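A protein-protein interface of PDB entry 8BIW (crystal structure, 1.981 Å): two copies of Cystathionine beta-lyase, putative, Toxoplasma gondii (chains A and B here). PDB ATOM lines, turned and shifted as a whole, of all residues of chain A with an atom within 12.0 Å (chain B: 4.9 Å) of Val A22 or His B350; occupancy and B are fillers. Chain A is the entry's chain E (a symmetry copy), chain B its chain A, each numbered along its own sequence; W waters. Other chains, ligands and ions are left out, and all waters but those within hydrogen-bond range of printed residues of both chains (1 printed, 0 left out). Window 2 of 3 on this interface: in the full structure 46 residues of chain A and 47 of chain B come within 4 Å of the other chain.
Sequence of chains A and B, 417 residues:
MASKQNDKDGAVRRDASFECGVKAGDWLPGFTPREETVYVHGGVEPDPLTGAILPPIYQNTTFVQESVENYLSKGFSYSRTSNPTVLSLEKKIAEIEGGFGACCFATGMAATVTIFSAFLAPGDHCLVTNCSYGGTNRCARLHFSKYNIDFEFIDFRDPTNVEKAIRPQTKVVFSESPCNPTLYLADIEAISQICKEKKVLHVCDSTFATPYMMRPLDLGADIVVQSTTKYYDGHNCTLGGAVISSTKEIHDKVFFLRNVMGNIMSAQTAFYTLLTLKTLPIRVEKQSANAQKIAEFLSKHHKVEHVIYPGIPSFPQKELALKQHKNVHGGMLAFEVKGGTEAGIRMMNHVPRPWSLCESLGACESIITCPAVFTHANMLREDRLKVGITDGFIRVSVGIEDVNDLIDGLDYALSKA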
ATOM      1  N   GLY A  21       8.884 -30.235 -24.376  1.00  0.00           N
ATOM      2  CA  GLY A  21       8.183 -30.127 -25.647  1.00  0.00           C
ATOM      3  C   GLY A  21       8.468 -28.887 -26.506  1.00  0.00           C
ATOM      4  O   GLY A  21       7.577 -28.067 -26.731  1.00  0.00           O
ATOM      5  N   VAL A  22       9.705 -28.752 -27.003  1.00  0.00           N
ATOM      6  CA  VAL A  22      10.094 -27.685 -27.923  1.00  0.00           C
ATOM      7  C   VAL A  22      10.728 -28.302 -29.162  1.00  0.00           C
ATOM      8  O   VAL A  22      11.389 -29.345 -29.100  1.00  0.00           O
ATOM      9  CB  VAL A  22      11.063 -26.696 -27.267  1.00  0.00           C
ATOM     10  CG1 VAL A  22      10.380 -25.990 -26.135  1.00  0.00           C
ATOM     11  CG2 VAL A  22      12.206 -27.462 -26.758  1.00  0.00           C
ATOM     12  N   LYS A  23      10.526 -27.637 -30.294  1.00  0.00           N
ATOM     13  CA  LYS A  23      10.771 -28.182 -31.615  1.00  0.00           C
ATOM     14  C   LYS A  23      11.786 -27.295 -32.345  1.00  0.00           C
ATOM     15  O   LYS A  23      12.168 -26.210 -31.872  1.00  0.00           O
ATOM     16  CB  LYS A  23       9.443 -28.291 -32.404  1.00  0.00           C
ATOM     17  N   ALA A  24      12.249 -27.788 -33.495  1.00  0.00           N
ATOM     18  CA  ALA A  24      13.088 -27.020 -34.403  1.00  0.00           C
ATOM     19  C   ALA A  24      12.602 -25.573 -34.517  1.00  0.00           C
ATOM     20  O   ALA A  24      11.412 -25.318 -34.634  1.00  0.00           O
ATOM     21  CB  ALA A  24      13.098 -27.701 -35.776  1.00  0.00           C
ATOM     22  N   GLY A  25      13.522 -24.627 -34.419  1.00  0.00           N
ATOM     23  CA  GLY A  25      13.188 -23.224 -34.567  1.00  0.00           C
ATOM     24  C   GLY A  25      12.883 -22.478 -33.282  1.00  0.00           C
ATOM     25  O   GLY A  25      12.703 -21.249 -33.338  1.00  0.00           O
ATOM     26  N   ASP A  26      12.795 -23.175 -32.138  1.00  0.00           N
ATOM     27  CA  ASP A  26      12.635 -22.590 -30.807  1.00  0.00           C
ATOM     28  C   ASP A  26      13.985 -22.583 -30.103  1.00  0.00           C
ATOM     29  O   ASP A  26      14.756 -23.540 -30.240  1.00  0.00           O
ATOM     30  CB  ASP A  26      11.684 -23.415 -29.912  1.00  0.00           C
ATOM     31  CG  ASP A  26      10.336 -23.737 -30.558  1.00  0.00           C
ATOM     32  OD1 ASP A  26       9.808 -22.839 -31.254  1.00  0.00           O
ATOM     33  OD2 ASP A  26       9.782 -24.863 -30.311  1.00  0.00           O
ATOM     34  N   TRP A  27      14.252 -21.539 -29.313  1.00  0.00           N
ATOM     35  CA  TRP A  27      15.256 -21.673 -28.267  1.00  0.00           C
ATOM     36  C   TRP A  27      14.678 -22.564 -27.167  1.00  0.00           C
ATOM     37  O   TRP A  27      13.468 -22.619 -26.970  1.00  0.00           O
ATOM     38  CB  TRP A  27      15.626 -20.305 -27.666  1.00  0.00           C
ATOM     39  CG  TRP A  27      16.223 -19.359 -28.673  1.00  0.00           C
ATOM     40  CD1 TRP A  27      15.549 -18.413 -29.409  1.00  0.00           C
ATOM     41  CD2 TRP A  27      17.598 -19.297 -29.095  1.00  0.00           C
ATOM     42  NE1 TRP A  27      16.428 -17.745 -30.252  1.00  0.00           N
ATOM     43  CE2 TRP A  27      17.691 -18.253 -30.068  1.00  0.00           C
ATOM     44  CE3 TRP A  27      18.761 -19.998 -28.734  1.00  0.00           C
ATOM     45  CZ2 TRP A  27      18.895 -17.909 -30.693  1.00  0.00           C
ATOM     46  CZ3 TRP A  27      19.965 -19.652 -29.347  1.00  0.00           C
ATOM     47  CH2 TRP A  27      20.032 -18.610 -30.323  1.00  0.00           C
ATOM     48  N   LEU A  28      15.535 -23.276 -26.455  1.00  0.00           N
ATOM     49  CA  LEU A  28      15.050 -24.030 -25.285  1.00  0.00           C
ATOM     50  C   LEU A  28      14.648 -23.031 -24.201  1.00  0.00           C
ATOM     51  O   LEU A  28      15.457 -22.178 -23.832  1.00  0.00           O
ATOM     52  CB  LEU A  28      16.152 -24.959 -24.760  1.00  0.00           C
ATOM     53  CG  LEU A  28      16.551 -26.161 -25.648  1.00  0.00           C
ATOM     54  CD1 LEU A  28      17.354 -27.154 -24.861  1.00  0.00           C
ATOM     55  CD2 LEU A  28      15.338 -26.834 -26.191  1.00  0.00           C
ATOM     56  N   PRO A  29      13.434 -23.091 -23.662  1.00  0.00           N
ATOM     57  CA  PRO A  29      13.056 -22.087 -22.651  1.00  0.00           C
ATOM     58  C   PRO A  29      13.880 -22.248 -21.381  1.00  0.00           C
ATOM     59  O   PRO A  29      14.246 -23.362 -20.998  1.00  0.00           O
ATOM     60  CB  PRO A  29      11.568 -22.357 -22.398  1.00  0.00           C
ATOM     61  CG  PRO A  29      11.284 -23.678 -22.975  1.00  0.00           C
ATOM     62  CD  PRO A  29      12.327 -24.012 -23.998  1.00  0.00           C
ATOM     63  N   GLY A  30      14.234 -21.119 -20.773  1.00  0.00           N
ATOM     64  CA  GLY A  30      14.981 -21.116 -19.537  1.00  0.00           C
ATOM     65  C   GLY A  30      16.481 -21.078 -19.710  1.00  0.00           C
ATOM     66  O   GLY A  30      17.210 -20.954 -18.719  1.00  0.00           O
ATOM     67  N   PHE A  31      16.979 -21.167 -20.929  1.00  0.00           N
ATOM     68  CA  PHE A  31      18.409 -21.132 -21.172  1.00  0.00           C
ATOM     69  C   PHE A  31      18.782 -19.790 -21.788  1.00  0.00           C
ATOM     70  O   PHE A  31      18.018 -19.233 -22.575  1.00  0.00           O
ATOM     71  CB  PHE A  31      18.803 -22.263 -22.128  1.00  0.00           C
ATOM     72  CG  PHE A  31      18.662 -23.641 -21.527  1.00  0.00           C
ATOM     73  CD1 PHE A  31      17.460 -24.304 -21.575  1.00  0.00           C
ATOM     74  CD2 PHE A  31      19.741 -24.261 -20.933  1.00  0.00           C
ATOM     75  CE1 PHE A  31      17.323 -25.574 -21.025  1.00  0.00           C
ATOM     76  CE2 PHE A  31      19.619 -25.525 -20.399  1.00  0.00           C
ATOM     77  CZ  PHE A  31      18.396 -26.180 -20.448  1.00  0.00           C
ATOM     78  N   ARG B 346      12.673 -37.679 -36.062  1.00  0.00           N
ATOM     79  CA  ARG B 346      12.357 -37.118 -34.742  1.00  0.00           C
ATOM     80  C   ARG B 346      13.498 -36.229 -34.235  1.00  0.00           C
ATOM     81  O   ARG B 346      13.274 -35.159 -33.638  1.00  0.00           O
ATOM     82  CB  ARG B 346      12.078 -38.256 -33.748  1.00  0.00           C
ATOM     83  CG  ARG B 346      11.290 -37.849 -32.480  1.00  0.00           C
ATOM     84  CD  ARG B 346      10.392 -39.016 -31.971  1.00  0.00           C
ATOM     85  NE  ARG B 346      11.120 -40.272 -32.090  1.00  0.00           N
ATOM     86  CZ  ARG B 346      10.704 -41.354 -32.750  1.00  0.00           C
ATOM     87  NH1 ARG B 346       9.517 -41.367 -33.344  1.00  0.00           N
ATOM     88  NH2 ARG B 346      11.483 -42.437 -32.801  1.00  0.00           N
ATOM     89  N   MET B 347      14.735 -36.665 -34.458  1.00  0.00           N
ATOM     90  CA  MET B 347      15.874 -35.865 -34.019  1.00  0.00           C
ATOM     91  C   MET B 347      15.850 -34.517 -34.727  1.00  0.00           C
ATOM     92  O   MET B 347      15.826 -33.454 -34.088  1.00  0.00           O
ATOM     93  CB  MET B 347      17.165 -36.634 -34.301  1.00  0.00           C
ATOM     94  CG  MET B 347      18.437 -36.153 -33.543  1.00  0.00           C
ATOM     95  SD  MET B 347      19.305 -35.110 -34.667  1.00  0.00           S
ATOM     96  CE  MET B 347      20.576 -34.444 -33.549  1.00  0.00           C
ATOM     97  N   MET B 348      15.731 -34.544 -36.054  1.00  0.00           N
ATOM     98  CA  MET B 348      15.804 -33.285 -36.779  1.00  0.00           C
ATOM     99  C   MET B 348      14.637 -32.365 -36.459  1.00  0.00           C
ATOM    100  O   MET B 348      14.811 -31.145 -36.426  1.00  0.00           O
ATOM    101  CB  MET B 348      15.923 -33.558 -38.272  1.00  0.00           C
ATOM    102  CG  MET B 348      17.426 -33.601 -38.674  1.00  0.00           C
ATOM    103  SD  MET B 348      17.613 -34.064 -40.385  1.00  0.00           S
ATOM    104  CE  MET B 348      16.821 -35.689 -40.494  1.00  0.00           C
ATOM    105  N   ASN B 349      13.453 -32.913 -36.199  1.00  0.00           N
ATOM    106  CA  ASN B 349      12.328 -32.087 -35.813  1.00  0.00           C
ATOM    107  C   ASN B 349      12.470 -31.505 -34.416  1.00  0.00           C
ATOM    108  O   ASN B 349      11.663 -30.650 -34.036  1.00  0.00           O
ATOM    109  CB  ASN B 349      11.059 -32.920 -35.881  1.00  0.00           C
ATOM    110  CG  ASN B 349      10.625 -33.174 -37.315  1.00  0.00           C
ATOM    111  OD1 ASN B 349      11.219 -32.648 -38.269  1.00  0.00           O
ATOM    112  ND2 ASN B 349       9.654 -34.054 -37.477  1.00  0.00           N
ATOM    113  N   HIS B 350      13.423 -31.985 -33.618  1.00  0.00           N
ATOM    114  CA  HIS B 350      13.592 -31.403 -32.293  1.00  0.00           C
ATOM    115  C   HIS B 350      14.922 -30.671 -32.127  1.00  0.00           C
ATOM    116  O   HIS B 350      15.334 -30.418 -30.989  1.00  0.00           O
ATOM    117  CB  HIS B 350      13.471 -32.489 -31.220  1.00  0.00           C
ATOM    118  CG  HIS B 350      12.072 -32.994 -31.046  1.00  0.00           C
ATOM    119  ND1 HIS B 350      11.505 -33.908 -31.909  1.00  0.00           N
ATOM    120  CD2 HIS B 350      11.121 -32.701 -30.123  1.00  0.00           C
ATOM    121  CE1 HIS B 350      10.257 -34.147 -31.534  1.00  0.00           C
ATOM    122  NE2 HIS B 350      10.005 -33.439 -30.446  1.00  0.00           N
ATOM    123  N   VAL B 351      15.632 -30.356 -33.212  1.00  0.00           N
ATOM    124  CA  VAL B 351      16.912 -29.694 -32.955  1.00  0.00           C
ATOM    125  C   VAL B 351      16.583 -28.215 -32.723  1.00  0.00           C
ATOM    126  O   VAL B 351      15.934 -27.567 -33.566  1.00  0.00           O
ATOM    127  CB  VAL B 351      17.953 -29.906 -34.076  1.00  0.00           C
ATOM    128  CG1 VAL B 351      19.344 -29.322 -33.628  1.00  0.00           C
ATOM    129  CG2 VAL B 351      18.167 -31.377 -34.359  1.00  0.00           C
ATOM    130  N   PRO B 352      16.956 -27.656 -31.586  1.00  0.00           N
ATOM    131  CA  PRO B 352      16.543 -26.294 -31.262  1.00  0.00           C
ATOM    132  C   PRO B 352      17.541 -25.268 -31.787  1.00  0.00           C
ATOM    133  O   PRO B 352      18.657 -25.588 -32.200  1.00  0.00           O
ATOM    134  CB  PRO B 352      16.535 -26.300 -29.725  1.00  0.00           C
ATOM    135  CG  PRO B 352      17.757 -27.162 -29.410  1.00  0.00           C
ATOM    136  CD  PRO B 352      17.728 -28.272 -30.472  1.00  0.00           C
ATOM    137  N   TYR B 412      20.049 -32.365 -26.638  1.00  0.00           N
ATOM    138  CA  TYR B 412      18.601 -32.312 -26.456  1.00  0.00           C
ATOM    139  C   TYR B 412      17.905 -33.086 -27.573  1.00  0.00           C
ATOM    140  O   TYR B 412      17.085 -33.990 -27.326  1.00  0.00           O
ATOM    141  CB  TYR B 412      18.134 -30.833 -26.427  1.00  0.00           C
ATOM    142  CG  TYR B 412      16.625 -30.734 -26.458  1.00  0.00           C
ATOM    143  CD1 TYR B 412      15.865 -30.817 -25.282  1.00  0.00           C
ATOM    144  CD2 TYR B 412      15.957 -30.626 -27.644  1.00  0.00           C
ATOM    145  CE1 TYR B 412      14.478 -30.794 -25.308  1.00  0.00           C
ATOM    146  CE2 TYR B 412      14.541 -30.574 -27.683  1.00  0.00           C
ATOM    147  CZ  TYR B 412      13.822 -30.647 -26.501  1.00  0.00           C
ATOM    148  OH  TYR B 412      12.448 -30.614 -26.533  1.00  0.00           O
ATOM    149  N   ALA B 413      18.261 -32.781 -28.826  1.00  0.00           N
ATOM    150  CA  ALA B 413      17.561 -33.436 -29.930  1.00  0.00           C
ATOM    151  C   ALA B 413      17.759 -34.950 -29.890  1.00  0.00           C
ATOM    152  O   ALA B 413      16.837 -35.712 -30.193  1.00  0.00           O
ATOM    153  CB  ALA B 413      18.049 -32.878 -31.282  1.00  0.00           C
ATOM    154  N   LYS B 416      15.616 -36.659 -27.450  1.00  0.00           N
ATOM    155  CA  LYS B 416      14.258 -36.819 -27.945  1.00  0.00           C
ATOM    156  C   LYS B 416      14.142 -37.853 -29.048  1.00  0.00           C
ATOM    157  O   LYS B 416      13.038 -38.331 -29.304  1.00  0.00           O
ATOM    158  CB  LYS B 416      13.703 -35.502 -28.506  1.00  0.00           C
ATOM    159  CG  LYS B 416      13.607 -34.369 -27.534  1.00  0.00           C
ATOM    160  CD  LYS B 416      12.697 -34.695 -26.384  1.00  0.00           C
ATOM    161  CE  LYS B 416      11.264 -34.409 -26.755  1.00  0.00           C
ATOM    162  NZ  LYS B 416      10.386 -34.632 -25.567  1.00  0.00           N
HETATM  163  O   HOH W   1      16.190 -25.177 -34.949  1.00  0.00           O
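OH of Tyr B412 is in hydrogen-bond range of O of Val A22, 3.1 Å away. O of Asn B349 is in hydrogen-bond range of N of Ala A24, 3.0 Å away.
OD2 of Asp A26 is in hydrogen-bond range of N of Lys A23 (2.9 Å). O of Arg B346 is in hydrogen-bond range of ND1 of His B350.
Among the printed residues, pairs that only touch across the chains: Val A22 with His B350, Lys A23 with Asn B349, Ala A24 with Met B348, Ala A24 with Val B351, Gly A25 with Val B351, Asp A26 with Pro B352, Leu A28 with Pro B352 and Leu A28 with Tyr B412.
Gly A21 touches none of the printed residues of chain B. Val A22 touches two residues of chain B. Of the printed residues of chain B, Lys A23 touches Asn B349. Printed residues of chain B within 4 Å of Asp A26: Pro B352. Of the printed residues of chain B, Leu A28 touches Pro B352 and Tyr B412. Gly A30 touches none of the printed residues of chain B. Of chain A, only Lys A23 and Ala A24 come within 4 Å of Asn B349. His B350 touches one residue of chain A. Pro B352 touches two residues of chain A. Of chain A, only Val A22 (3.1 Å) and Leu A28 (3.98 Å) come within 4 Å of Tyr B412. No residue of chain A comes within 4 Å of Lys B416. The nearest printed residue of chain B that does not touch Ala A24 is His B350 (4.04 Å).
Of the 10 printed residues of chain B, 6 touch a printed residue of chain A. Printed residues of chain B that touch a printed residue of chain A: Met B348, Asn B349, His B350, Val B351, Pro B352 and Tyr B412. Hydrophobic or aromatic side chains of chain B within 4 Å of the printed part of chain A: His B350, Pro B352 and Tyr B412. Among the printed residues, no Asp or Glu carboxylate lies within 4 Å of a Lys or Arg side-chain nitrogen of the other chain.
No position is printed for both chains. Of the 10 pairs that touch across the chains among the printed residues, none has its exchanged pair printed and touching as well.
Water W1 bridges the backbone carbonyl oxygen (O) of Val B351 and the backbone NH (N) of Gly A25.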
